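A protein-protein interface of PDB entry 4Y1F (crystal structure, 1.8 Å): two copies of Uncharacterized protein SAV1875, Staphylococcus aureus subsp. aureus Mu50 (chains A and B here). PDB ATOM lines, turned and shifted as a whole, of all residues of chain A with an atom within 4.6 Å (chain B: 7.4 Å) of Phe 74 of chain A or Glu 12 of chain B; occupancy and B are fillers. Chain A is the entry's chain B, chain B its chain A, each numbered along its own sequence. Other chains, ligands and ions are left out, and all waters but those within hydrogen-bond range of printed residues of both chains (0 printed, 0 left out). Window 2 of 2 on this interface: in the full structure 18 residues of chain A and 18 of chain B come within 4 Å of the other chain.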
ATOM      1  N   ASN A  11       8.318  20.347  10.712  1.00  0.00           N
ATOM      2  CA  ASN A  11       7.539  21.534  10.391  1.00  0.00           C
ATOM      3  C   ASN A  11       6.106  21.251   9.958  1.00  0.00           C
ATOM      4  O   ASN A  11       5.786  20.129   9.567  1.00  0.00           O
ATOM      5  CB  ASN A  11       8.263  22.403   9.372  1.00  0.00           C
ATOM      6  CG  ASN A  11       9.501  23.048   9.951  1.00  0.00           C
ATOM      7  OD1 ASN A  11       9.415  23.936  10.802  1.00  0.00           O
ATOM      8  ND2 ASN A  11      10.665  22.595   9.503  1.00  0.00           N
ATOM      9  N   GLU A  12       5.230  22.215  10.250  1.00  0.00           N
ATOM     10  CA  GLU A  12       3.817  22.195   9.863  1.00  0.00           C
ATOM     11  C   GLU A  12       3.006  21.150  10.599  1.00  0.00           C
ATOM     12  O   GLU A  12       2.015  20.633  10.071  1.00  0.00           O
ATOM     13  CB  GLU A  12       3.648  22.070   8.346  1.00  0.00           C
ATOM     14  CG  GLU A  12       4.256  23.240   7.577  1.00  0.00           C
ATOM     15  CD  GLU A  12       4.167  23.061   6.074  1.00  0.00           C
ATOM     16  OE1 GLU A  12       4.946  22.248   5.520  1.00  0.00           O
ATOM     17  OE2 GLU A  12       3.277  23.685   5.458  1.00  0.00           O
ATOM     18  N   LYS A  46       1.637  24.855  11.783  1.00  0.00           N
ATOM     19  CA  LYS A  46       0.855  25.466  10.693  1.00  0.00           C
ATOM     20  C   LYS A  46       0.379  26.853  11.077  1.00  0.00           C
ATOM     21  O   LYS A  46       0.119  27.676  10.210  1.00  0.00           O
ATOM     22  CB  LYS A  46      -0.356  24.586  10.363  1.00  0.00           C
ATOM     23  CG  LYS A  46       0.015  23.275   9.696  1.00  0.00           C
ATOM     24  CD  LYS A  46      -1.134  22.280   9.707  1.00  0.00           C
ATOM     25  CE  LYS A  46      -2.111  22.566   8.586  1.00  0.00           C
ATOM     26  NZ  LYS A  46      -2.685  21.289   8.074  1.00  0.00           N
ATOM     27  N   GLY A  72      -0.239  15.586  14.629  1.00  0.00           N
ATOM     28  CA  GLY A  72      -0.699  15.557  13.243  1.00  0.00           C
ATOM     29  C   GLY A  72      -0.286  16.782  12.452  1.00  0.00           C
ATOM     30  O   GLY A  72       0.841  17.270  12.575  1.00  0.00           O
ATOM     31  N   GLY A  73      -1.151  17.196  11.537  1.00  0.00           N
ATOM     32  CA  GLY A  73      -0.768  18.203  10.569  1.00  0.00           C
ATOM     33  C   GLY A  73      -0.028  17.554   9.421  1.00  0.00           C
ATOM     34  O   GLY A  73      -0.172  16.359   9.187  1.00  0.00           O
ATOM     35  N   PHE A  74       0.856  18.312   8.795  1.00  0.00           N
ATOM     36  CA  PHE A  74       1.734  17.784   7.765  1.00  0.00           C
ATOM     37  C   PHE A  74       3.114  17.417   8.280  1.00  0.00           C
ATOM     38  O   PHE A  74       3.964  16.948   7.505  1.00  0.00           O
ATOM     39  CB  PHE A  74       1.855  18.776   6.614  1.00  0.00           C
ATOM     40  CG  PHE A  74       0.559  18.992   5.887  1.00  0.00           C
ATOM     41  CD1 PHE A  74      -0.250  17.901   5.569  1.00  0.00           C
ATOM     42  CD2 PHE A  74       0.047  20.268   5.724  1.00  0.00           C
ATOM     43  CE1 PHE A  74      -1.481  18.081   4.946  1.00  0.00           C
ATOM     44  CE2 PHE A  74      -1.145  20.453   5.039  1.00  0.00           C
ATOM     45  CZ  PHE A  74      -1.954  19.364   4.759  1.00  0.00           C
ATOM     46  N   SER A  75       3.271  17.439   9.606  1.00  0.00           N
ATOM     47  CA  SER A  75       4.508  16.945  10.223  1.00  0.00           C
ATOM     48  C   SER A  75       4.763  15.444   9.917  1.00  0.00           C
ATOM     49  O   SER A  75       5.839  15.077   9.442  1.00  0.00           O
ATOM     50  CB  SER A  75       4.471  17.217  11.747  1.00  0.00           C
ATOM     51  OG  SER A  75       5.539  16.548  12.393  1.00  0.00           O
ATOM     52  N   PRO A  76       3.730  14.584  10.072  1.00  0.00           N
ATOM     53  CA  PRO A  76       3.993  13.181   9.765  1.00  0.00           C
ATOM     54  C   PRO A  76       4.408  12.944   8.326  1.00  0.00           C
ATOM     55  O   PRO A  76       5.334  12.180   8.068  1.00  0.00           O
ATOM     56  CB  PRO A  76       2.649  12.500  10.063  1.00  0.00           C
ATOM     57  CG  PRO A  76       2.064  13.328  11.145  1.00  0.00           C
ATOM     58  CD  PRO A  76       2.510  14.750  10.883  1.00  0.00           C
ATOM     59  N   ASP A  77       3.807  13.668   7.391  1.00  0.00           N
ATOM     60  CA  ASP A  77       4.270  13.553   6.014  1.00  0.00           C
ATOM     61  C   ASP A  77       5.732  13.937   5.841  1.00  0.00           C
ATOM     62  O   ASP A  77       6.492  13.243   5.157  1.00  0.00           O
ATOM     63  CB  ASP A  77       3.413  14.375   5.061  1.00  0.00           C
ATOM     64  CG  ASP A  77       3.645  13.992   3.601  1.00  0.00           C
ATOM     65  OD1 ASP A  77       2.870  13.188   3.058  1.00  0.00           O
ATOM     66  OD2 ASP A  77       4.549  14.571   2.978  1.00  0.00           O
ATOM     67  N   HIS A  78       6.121  15.065   6.416  1.00  0.00           N
ATOM     68  CA  HIS A  78       7.509  15.472   6.401  1.00  0.00           C
ATOM     69  C   HIS A  78       8.418  14.392   6.973  1.00  0.00           C
ATOM     70  O   HIS A  78       9.477  14.074   6.399  1.00  0.00           O
ATOM     71  CB  HIS A  78       7.671  16.781   7.148  1.00  0.00           C
ATOM     72  CG  HIS A  78       7.162  17.993   6.386  1.00  0.00           C
ATOM     73  ND1 HIS A  78       7.475  18.215   5.089  1.00  0.00           N
ATOM     74  CD2 HIS A  78       6.454  19.125   6.820  1.00  0.00           C
ATOM     75  CE1 HIS A  78       6.933  19.397   4.689  1.00  0.00           C
ATOM     76  NE2 HIS A  78       6.303  19.948   5.747  1.00  0.00           N
ATOM     77  N   HIS A 106      -3.375  13.226  11.424  1.00  0.00           N
ATOM     78  CA  HIS A 106      -2.479  12.544  10.476  1.00  0.00           C
ATOM     79  C   HIS A 106      -1.403  11.717  11.111  1.00  0.00           C
ATOM     80  O   HIS A 106      -0.684  10.986  10.422  1.00  0.00           O
ATOM     81  CB  HIS A 106      -1.787  13.551   9.556  1.00  0.00           C
ATOM     82  CG  HIS A 106      -2.685  14.135   8.510  1.00  0.00           C
ATOM     83  ND1 HIS A 106      -3.513  15.153   8.775  1.00  0.00           N
ATOM     84  CD2 HIS A 106      -2.684  13.981   7.120  1.00  0.00           C
ATOM     85  CE1 HIS A 106      -4.130  15.538   7.634  1.00  0.00           C
ATOM     86  NE2 HIS A 106      -3.646  14.789   6.629  1.00  0.00           N
ATOM     87  N   LEU B   9      -7.269  20.351  -8.031  1.00  0.00           N
ATOM     88  CA  LEU B   9      -6.416  21.239  -7.262  1.00  0.00           C
ATOM     89  C   LEU B   9      -7.097  21.766  -5.996  1.00  0.00           C
ATOM     90  O   LEU B   9      -8.278  22.151  -6.018  1.00  0.00           O
ATOM     91  CB  LEU B   9      -5.941  22.413  -8.145  1.00  0.00           C
ATOM     92  CG  LEU B   9      -4.626  23.080  -7.810  1.00  0.00           C
ATOM     93  CD1 LEU B   9      -3.463  22.116  -8.052  1.00  0.00           C
ATOM     94  CD2 LEU B   9      -4.432  24.318  -8.680  1.00  0.00           C
ATOM     95  N   ALA B  10      -6.385  21.631  -4.878  1.00  0.00           N
ATOM     96  CA  ALA B  10      -6.771  22.226  -3.611  1.00  0.00           C
ATOM     97  C   ALA B  10      -5.679  23.192  -3.182  1.00  0.00           C
ATOM     98  O   ALA B  10      -4.630  23.315  -3.835  1.00  0.00           O
ATOM     99  CB  ALA B  10      -6.986  21.126  -2.558  1.00  0.00           C
ATOM    100  N   ASN B  11      -5.869  23.825  -2.031  1.00  0.00           N
ATOM    101  CA  ASN B  11      -4.828  24.696  -1.507  1.00  0.00           C
ATOM    102  C   ASN B  11      -3.558  23.901  -1.203  1.00  0.00           C
ATOM    103  O   ASN B  11      -3.608  22.690  -0.921  1.00  0.00           O
ATOM    104  CB  ASN B  11      -5.319  25.369  -0.207  1.00  0.00           C
ATOM    105  CG  ASN B  11      -6.365  26.423  -0.461  1.00  0.00           C
ATOM    106  OD1 ASN B  11      -6.077  27.472  -1.039  1.00  0.00           O
ATOM    107  ND2 ASN B  11      -7.602  26.141  -0.057  1.00  0.00           N
ATOM    108  N   GLU B  12      -2.434  24.610  -1.199  1.00  0.00           N
ATOM    109  CA  GLU B  12      -1.139  24.076  -0.792  1.00  0.00           C
ATOM    110  C   GLU B  12      -0.579  23.077  -1.788  1.00  0.00           C
ATOM    111  O   GLU B  12       0.254  22.225  -1.446  1.00  0.00           O
ATOM    112  CB  GLU B  12      -1.219  23.506   0.627  1.00  0.00           C
ATOM    113  CG  GLU B  12      -1.624  24.583   1.636  1.00  0.00           C
ATOM    114  CD  GLU B  12      -1.537  24.108   3.077  1.00  0.00           C
ATOM    115  OE1 GLU B  12      -2.554  23.614   3.618  1.00  0.00           O
ATOM    116  OE2 GLU B  12      -0.452  24.229   3.668  1.00  0.00           O
ATOM    117  N   PHE B  13      -0.998  23.213  -3.038  1.00  0.00           N
ATOM    118  CA  PHE B  13      -0.293  22.548  -4.116  1.00  0.00           C
ATOM    119  C   PHE B  13       1.148  23.074  -4.222  1.00  0.00           C
ATOM    120  O   PHE B  13       1.454  24.209  -3.800  1.00  0.00           O
ATOM    121  CB  PHE B  13      -1.061  22.692  -5.439  1.00  0.00           C
ATOM    122  CG  PHE B  13      -1.210  24.125  -5.910  1.00  0.00           C
ATOM    123  CD1 PHE B  13      -2.290  24.905  -5.494  1.00  0.00           C
ATOM    124  CD2 PHE B  13      -0.284  24.678  -6.788  1.00  0.00           C
ATOM    125  CE1 PHE B  13      -2.420  26.231  -5.893  1.00  0.00           C
ATOM    126  CE2 PHE B  13      -0.444  25.989  -7.240  1.00  0.00           C
ATOM    127  CZ  PHE B  13      -1.499  26.764  -6.787  1.00  0.00           C
ATOM    128  N   GLU B  14       2.049  22.201  -4.688  1.00  0.00           N
ATOM    129  CA  GLU B  14       3.411  22.608  -5.015  1.00  0.00           C
ATOM    130  C   GLU B  14       3.392  23.429  -6.318  1.00  0.00           C
ATOM    131  O   GLU B  14       2.970  22.934  -7.357  1.00  0.00           O
ATOM    132  CB  GLU B  14       4.297  21.356  -5.182  1.00  0.00           C
ATOM    133  CG  GLU B  14       5.763  21.664  -5.491  1.00  0.00           C
ATOM    134  CD  GLU B  14       6.489  22.295  -4.312  1.00  0.00           C
ATOM    135  OE1 GLU B  14       6.527  21.671  -3.235  1.00  0.00           O
ATOM    136  OE2 GLU B  14       7.072  23.393  -4.479  1.00  0.00           O
ATOM    137  N   ASP B  15       3.664  24.725  -6.210  1.00  0.00           N
ATOM    138  CA  ASP B  15       3.334  25.650  -7.280  1.00  0.00           C
ATOM    139  C   ASP B  15       3.852  25.122  -8.633  1.00  0.00           C
ATOM    140  O   ASP B  15       3.163  25.228  -9.637  1.00  0.00           O
ATOM    141  CB  ASP B  15       3.910  27.071  -7.024  1.00  0.00           C
ATOM    142  CG  ASP B  15       3.528  27.639  -5.655  1.00  0.00           C
ATOM    143  OD1 ASP B  15       3.470  26.870  -4.675  1.00  0.00           O
ATOM    144  OD2 ASP B  15       3.454  28.897  -5.523  1.00  0.00           O
ATOM    145  N   VAL B  43      -7.456  28.952  -5.044  1.00  0.00           N
ATOM    146  CA  VAL B  43      -6.573  28.129  -4.222  1.00  0.00           C
ATOM    147  C   VAL B  43      -5.147  28.649  -4.329  1.00  0.00           C
ATOM    148  O   VAL B  43      -4.780  29.316  -5.311  1.00  0.00           O
ATOM    149  CB  VAL B  43      -6.641  26.644  -4.609  1.00  0.00           C
ATOM    150  CG1 VAL B  43      -8.050  26.082  -4.378  1.00  0.00           C
ATOM    151  CG2 VAL B  43      -6.217  26.467  -6.059  1.00  0.00           C
ATOM    152  N   VAL B  44      -4.382  28.471  -3.259  1.00  0.00           N
ATOM    153  CA  VAL B  44      -3.104  29.158  -3.135  1.00  0.00           C
ATOM    154  C   VAL B  44      -2.027  28.132  -2.867  1.00  0.00           C
ATOM    155  O   VAL B  44      -2.187  27.281  -1.977  1.00  0.00           O
ATOM    156  CB  VAL B  44      -3.102  30.161  -1.958  1.00  0.00           C
ATOM    157  CG1 VAL B  44      -1.729  30.803  -1.845  1.00  0.00           C
ATOM    158  CG2 VAL B  44      -4.167  31.233  -2.184  1.00  0.00           C
ATOM    159  N   GLY B  45      -0.981  28.169  -3.685  1.00  0.00           N
ATOM    160  CA  GLY B  45       0.118  27.201  -3.595  1.00  0.00           C
ATOM    161  C   GLY B  45       0.974  27.400  -2.361  1.00  0.00           C
ATOM    162  O   GLY B  45       0.919  28.450  -1.709  1.00  0.00           O
ATOM    163  N   LYS B  46       1.777  26.390  -2.040  1.00  0.00           N
ATOM    164  CA  LYS B  46       2.727  26.481  -0.938  1.00  0.00           C
ATOM    165  C   LYS B  46       3.513  27.791  -0.973  1.00  0.00           C
ATOM    166  O   LYS B  46       3.827  28.365   0.068  1.00  0.00           O
ATOM    167  CB  LYS B  46       3.677  25.278  -0.956  1.00  0.00           C
ATOM    168  CG  LYS B  46       3.010  23.996  -0.481  1.00  0.00           C
ATOM    169  CD  LYS B  46       3.899  22.784  -0.721  1.00  0.00           C
ATOM    170  CE  LYS B  46       4.762  22.490   0.489  1.00  0.00           C
ATOM    171  NZ  LYS B  46       4.675  21.044   0.826  1.00  0.00           N
ATOM    172  N   HIS B  47       3.895  28.209  -2.169  1.00  0.00           N
ATOM    173  CA  HIS B  47       4.786  29.351  -2.334  1.00  0.00           C
ATOM    174  C   HIS B  47       4.040  30.553  -2.835  1.00  0.00           C
ATOM    175  O   HIS B  47       4.625  31.469  -3.402  1.00  0.00           O
ATOM    176  CB  HIS B  47       5.967  28.979  -3.234  1.00  0.00           C
ATOM    177  CG  HIS B  47       6.764  27.806  -2.712  1.00  0.00           C
ATOM    178  ND1 HIS B  47       7.256  27.782  -1.449  1.00  0.00           N
ATOM    179  CD2 HIS B  47       6.926  26.515  -3.214  1.00  0.00           C
ATOM    180  CE1 HIS B  47       7.737  26.554  -1.174  1.00  0.00           C
ATOM    181  NE2 HIS B  47       7.568  25.788  -2.266  1.00  0.00           N
ATOM    182  N   GLU B  49       1.415  31.028  -5.135  1.00  0.00           N
ATOM    183  CA  GLU B  49       0.771  31.170  -6.435  1.00  0.00           C
ATOM    184  C   GLU B  49      -0.751  31.028  -6.321  1.00  0.00           C
ATOM    185  O   GLU B  49      -1.262  30.073  -5.735  1.00  0.00           O
ATOM    186  CB  GLU B  49       1.305  30.145  -7.435  1.00  0.00           C
ATOM    187  CG  GLU B  49       0.512  30.132  -8.737  1.00  0.00           C
ATOM    188  CD  GLU B  49       1.264  29.491  -9.892  1.00  0.00           C
ATOM    189  OE1 GLU B  49       2.189  28.700  -9.623  1.00  0.00           O
ATOM    190  OE2 GLU B  49       0.857  29.692 -11.063  1.00  0.00           O
ATOM    191  N   GLY B  72       1.208  17.861  -7.115  1.00  0.00           N
ATOM    192  CA  GLY B  72       1.535  17.432  -5.744  1.00  0.00           C
ATOM    193  C   GLY B  72       1.538  18.578  -4.731  1.00  0.00           C
ATOM    194  O   GLY B  72       0.591  19.359  -4.652  1.00  0.00           O
ATOM    195  N   GLY B  73       2.469  18.513  -3.787  1.00  0.00           N
ATOM    196  CA  GLY B  73       2.316  19.262  -2.537  1.00  0.00           C
ATOM    197  C   GLY B  73       1.292  18.638  -1.606  1.00  0.00           C
ATOM    198  O   GLY B  73       1.147  17.423  -1.565  1.00  0.00           O
ATOM    199  N   PHE B  74       0.635  19.472  -0.803  1.00  0.00           N
ATOM    200  CA  PHE B  74      -0.400  18.972   0.093  1.00  0.00           C
ATOM    201  C   PHE B  74      -1.806  19.131  -0.462  1.00  0.00           C
ATOM    202  O   PHE B  74      -2.772  18.705   0.178  1.00  0.00           O
ATOM    203  CB  PHE B  74      -0.271  19.614   1.464  1.00  0.00           C
ATOM    204  CG  PHE B  74       1.041  19.305   2.124  1.00  0.00           C
ATOM    205  CD1 PHE B  74       1.444  17.985   2.279  1.00  0.00           C
ATOM    206  CD2 PHE B  74       1.867  20.314   2.565  1.00  0.00           C
ATOM    207  CE1 PHE B  74       2.671  17.683   2.849  1.00  0.00           C
ATOM    208  CE2 PHE B  74       3.042  20.017   3.230  1.00  0.00           C
ATOM    209  CZ  PHE B  74       3.490  18.708   3.274  1.00  0.00           C
ATOM    210  N   SER B  75      -1.890  19.500  -1.749  1.00  0.00           N
ATOM    211  CA  SER B  75      -3.172  19.496  -2.455  1.00  0.00           C
ATOM    212  C   SER B  75      -3.876  18.129  -2.502  1.00  0.00           C
ATOM    213  O   SER B  75      -5.060  18.001  -2.094  1.00  0.00           O
ATOM    214  CB  SER B  75      -3.030  20.155  -3.851  1.00  0.00           C
ATOM    215  OG  SER B  75      -4.178  19.898  -4.667  1.00  0.00           O
ATOM    216  N   PRO B  76      -3.136  17.064  -2.867  1.00  0.00           N
ATOM    217  CA  PRO B  76      -3.820  15.786  -2.868  1.00  0.00           C
ATOM    218  C   PRO B  76      -4.353  15.364  -1.491  1.00  0.00           C
ATOM    219  O   PRO B  76      -5.432  14.773  -1.399  1.00  0.00           O
ATOM    220  CB  PRO B  76      -2.747  14.807  -3.378  1.00  0.00           C
ATOM    221  CG  PRO B  76      -1.841  15.663  -4.237  1.00  0.00           C
ATOM    222  CD  PRO B  76      -1.795  16.995  -3.497  1.00  0.00           C
ATOM    223  N   ASP B  77      -3.617  15.660  -0.429  1.00  0.00           N
ATOM    224  CA  ASP B  77      -4.116  15.325   0.903  1.00  0.00           C
ATOM    225  C   ASP B  77      -5.402  16.062   1.202  1.00  0.00           C
ATOM    226  O   ASP B  77      -6.395  15.479   1.656  1.00  0.00           O
ATOM    227  CB  ASP B  77      -3.065  15.664   1.948  1.00  0.00           C
ATOM    228  CG  ASP B  77      -3.404  15.064   3.314  1.00  0.00           C
ATOM    229  OD1 ASP B  77      -2.810  14.021   3.672  1.00  0.00           O
ATOM    230  OD2 ASP B  77      -4.245  15.654   4.012  1.00  0.00           O
ATOM    231  N   HIS B  78      -5.420  17.355   0.905  1.00  0.00           N
ATOM    232  CA  HIS B  78      -6.666  18.097   0.983  1.00  0.00           C
ATOM    233  C   HIS B  78      -7.803  17.493   0.205  1.00  0.00           C
ATOM    234  O   HIS B  78      -8.928  17.423   0.711  1.00  0.00           O
ATOM    235  CB  HIS B  78      -6.440  19.542   0.579  1.00  0.00           C
ATOM    236  CG  HIS B  78      -5.667  20.328   1.608  1.00  0.00           C
ATOM    237  ND1 HIS B  78      -5.986  20.313   2.920  1.00  0.00           N
ATOM    238  CD2 HIS B  78      -4.567  21.169   1.478  1.00  0.00           C
ATOM    239  CE1 HIS B  78      -5.179  21.166   3.585  1.00  0.00           C
ATOM    240  NE2 HIS B  78      -4.315  21.695   2.698  1.00  0.00           N
ATOM    241  N   ASN B 127       7.772  10.017   0.250  1.00  0.00           N
ATOM    242  CA  ASN B 127       6.788  10.076   1.357  1.00  0.00           C
ATOM    243  C   ASN B 127       5.576   9.168   1.142  1.00  0.00           C
ATOM    244  O   ASN B 127       4.781   8.967   2.058  1.00  0.00           O
ATOM    245  CB  ASN B 127       6.244  11.510   1.546  1.00  0.00           C
ATOM    246  CG  ASN B 127       7.327  12.561   1.590  1.00  0.00           C
ATOM    247  OD1 ASN B 127       7.285  13.479   2.436  1.00  0.00           O
ATOM    248  ND2 ASN B 127       8.321  12.433   0.716  1.00  0.00           N
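Glu 12 of chain A touches Phe 74 of chain B, and with the chains exchanged Phe 74 of chain A touches Glu 12 of chain B.
Phe 74 of chain B touches its own counterpart, Phe 74 of chain A.
Phe 74 of chain A touches Asp 77 of chain B, and with the chains exchanged Asp 77 of chain A touches Phe 74 of chain B.
Phe 74 of chain A touches His 78 of chain B, and with the chains exchanged His 78 of chain A touches Phe 74 of chain B.
Positions printed for both chains: 11, 12, 46, 72, 73, 74, 75, 76, 77 and 78.
Hydrophobic or aromatic side chains of chain A that line the printed part of chain B: Phe 74, His 78 and His 106.
Of the 21 printed residues of chain B, 5 touch a printed residue of chain A.
Among the printed residues, no Asp or Glu carboxylate lies within 4 Å of a Lys or Arg side-chain nitrogen of the other chain.
The side-chain carboxylate of Asp 77 of chain B lies within hydrogen-bond range of a ring nitrogen (NE2) of His 106 of chain A, 2.8 Å away.
The side-chain amide oxygen (OD1) of Asn 127 of chain B sits close to the backbone carbonyl oxygen (O) of Asp 77 of chain A (2.8 Å).
Phe 74 of chain A touches just these residues of chain B: Glu 12 (3.7 Å), Phe 74 (3.6 Å), Asp 77 (3.8 Å) and His 78 (3.9 Å).
Glu 12 of chain B touches just one residue of chain A: Phe 74.
Of the printed residues of chain A, Asp 77 of chain B touches Phe 74 and His 106.
Of the printed residues of chain B, His 78 of chain A touches Phe 74.
Of the printed residues of chain A, Asn 127 of chain B touches Asp 77 (2.8 Å).
Of the printed residues of chain B, Glu 12 of chain A touches Phe 74 (3.7 Å).
Of the printed residues of chain A, Phe 74 of chain B touches Glu 12 (3.7 Å), Phe 74 (3.6 Å), Asp 77 (3.6 Å) and His 78 (3.8 Å).
Val 44 of chain B touches none of the printed residues of chain A.
The nearest residue of chain B that does not touch Phe 74 of chain A is Ser 75 of chain B (6.5 Å).
N of Glu 12 of chain B is in hydrogen-bond range of O of Val 44 of chain B, 2.8 Å away.
The backbone carbonyl oxygen of Glu 12 of chain B lies within hydrogen-bond range of the backbone NH of Phe 74 of chain B, at 2.9 Å.
The backbone carbonyl oxygen (O) of Glu 12 of chain B lies within hydrogen-bond range of the backbone NH (N) of Ser 75 of chain B, at 3.5 Å.
OE1 of Glu 12 of chain B is in hydrogen-bond range of NE2 of His 78 of chain B (2.8 Å).
The backbone NH (N) of Phe 74 of chain A sits at hydrogen-bond distance from the backbone carbonyl oxygen (O) of Glu 12 of chain A, 2.9 Å away.
The side-chain carboxylate (OE1) of Glu 12 of chain A is in hydrogen-bond range of a ring nitrogen (NE2) of His 78 of chain A, at 2.7 Å.
Among the printed residues, merely in contact across the chains: Asp 77 of chain A with Phe 74 of chain B, Phe 74 of chain A with Phe 74 of chain B, Glu 12 of chain A with Phe 74 of chain B, Phe 74 of chain A with Glu 12 of chain B, His 78 of chain A with Phe 74 of chain B, Phe 74 of chain A with Asp 77 of chain B and Phe 74 of chain A with His 78 of chain B.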
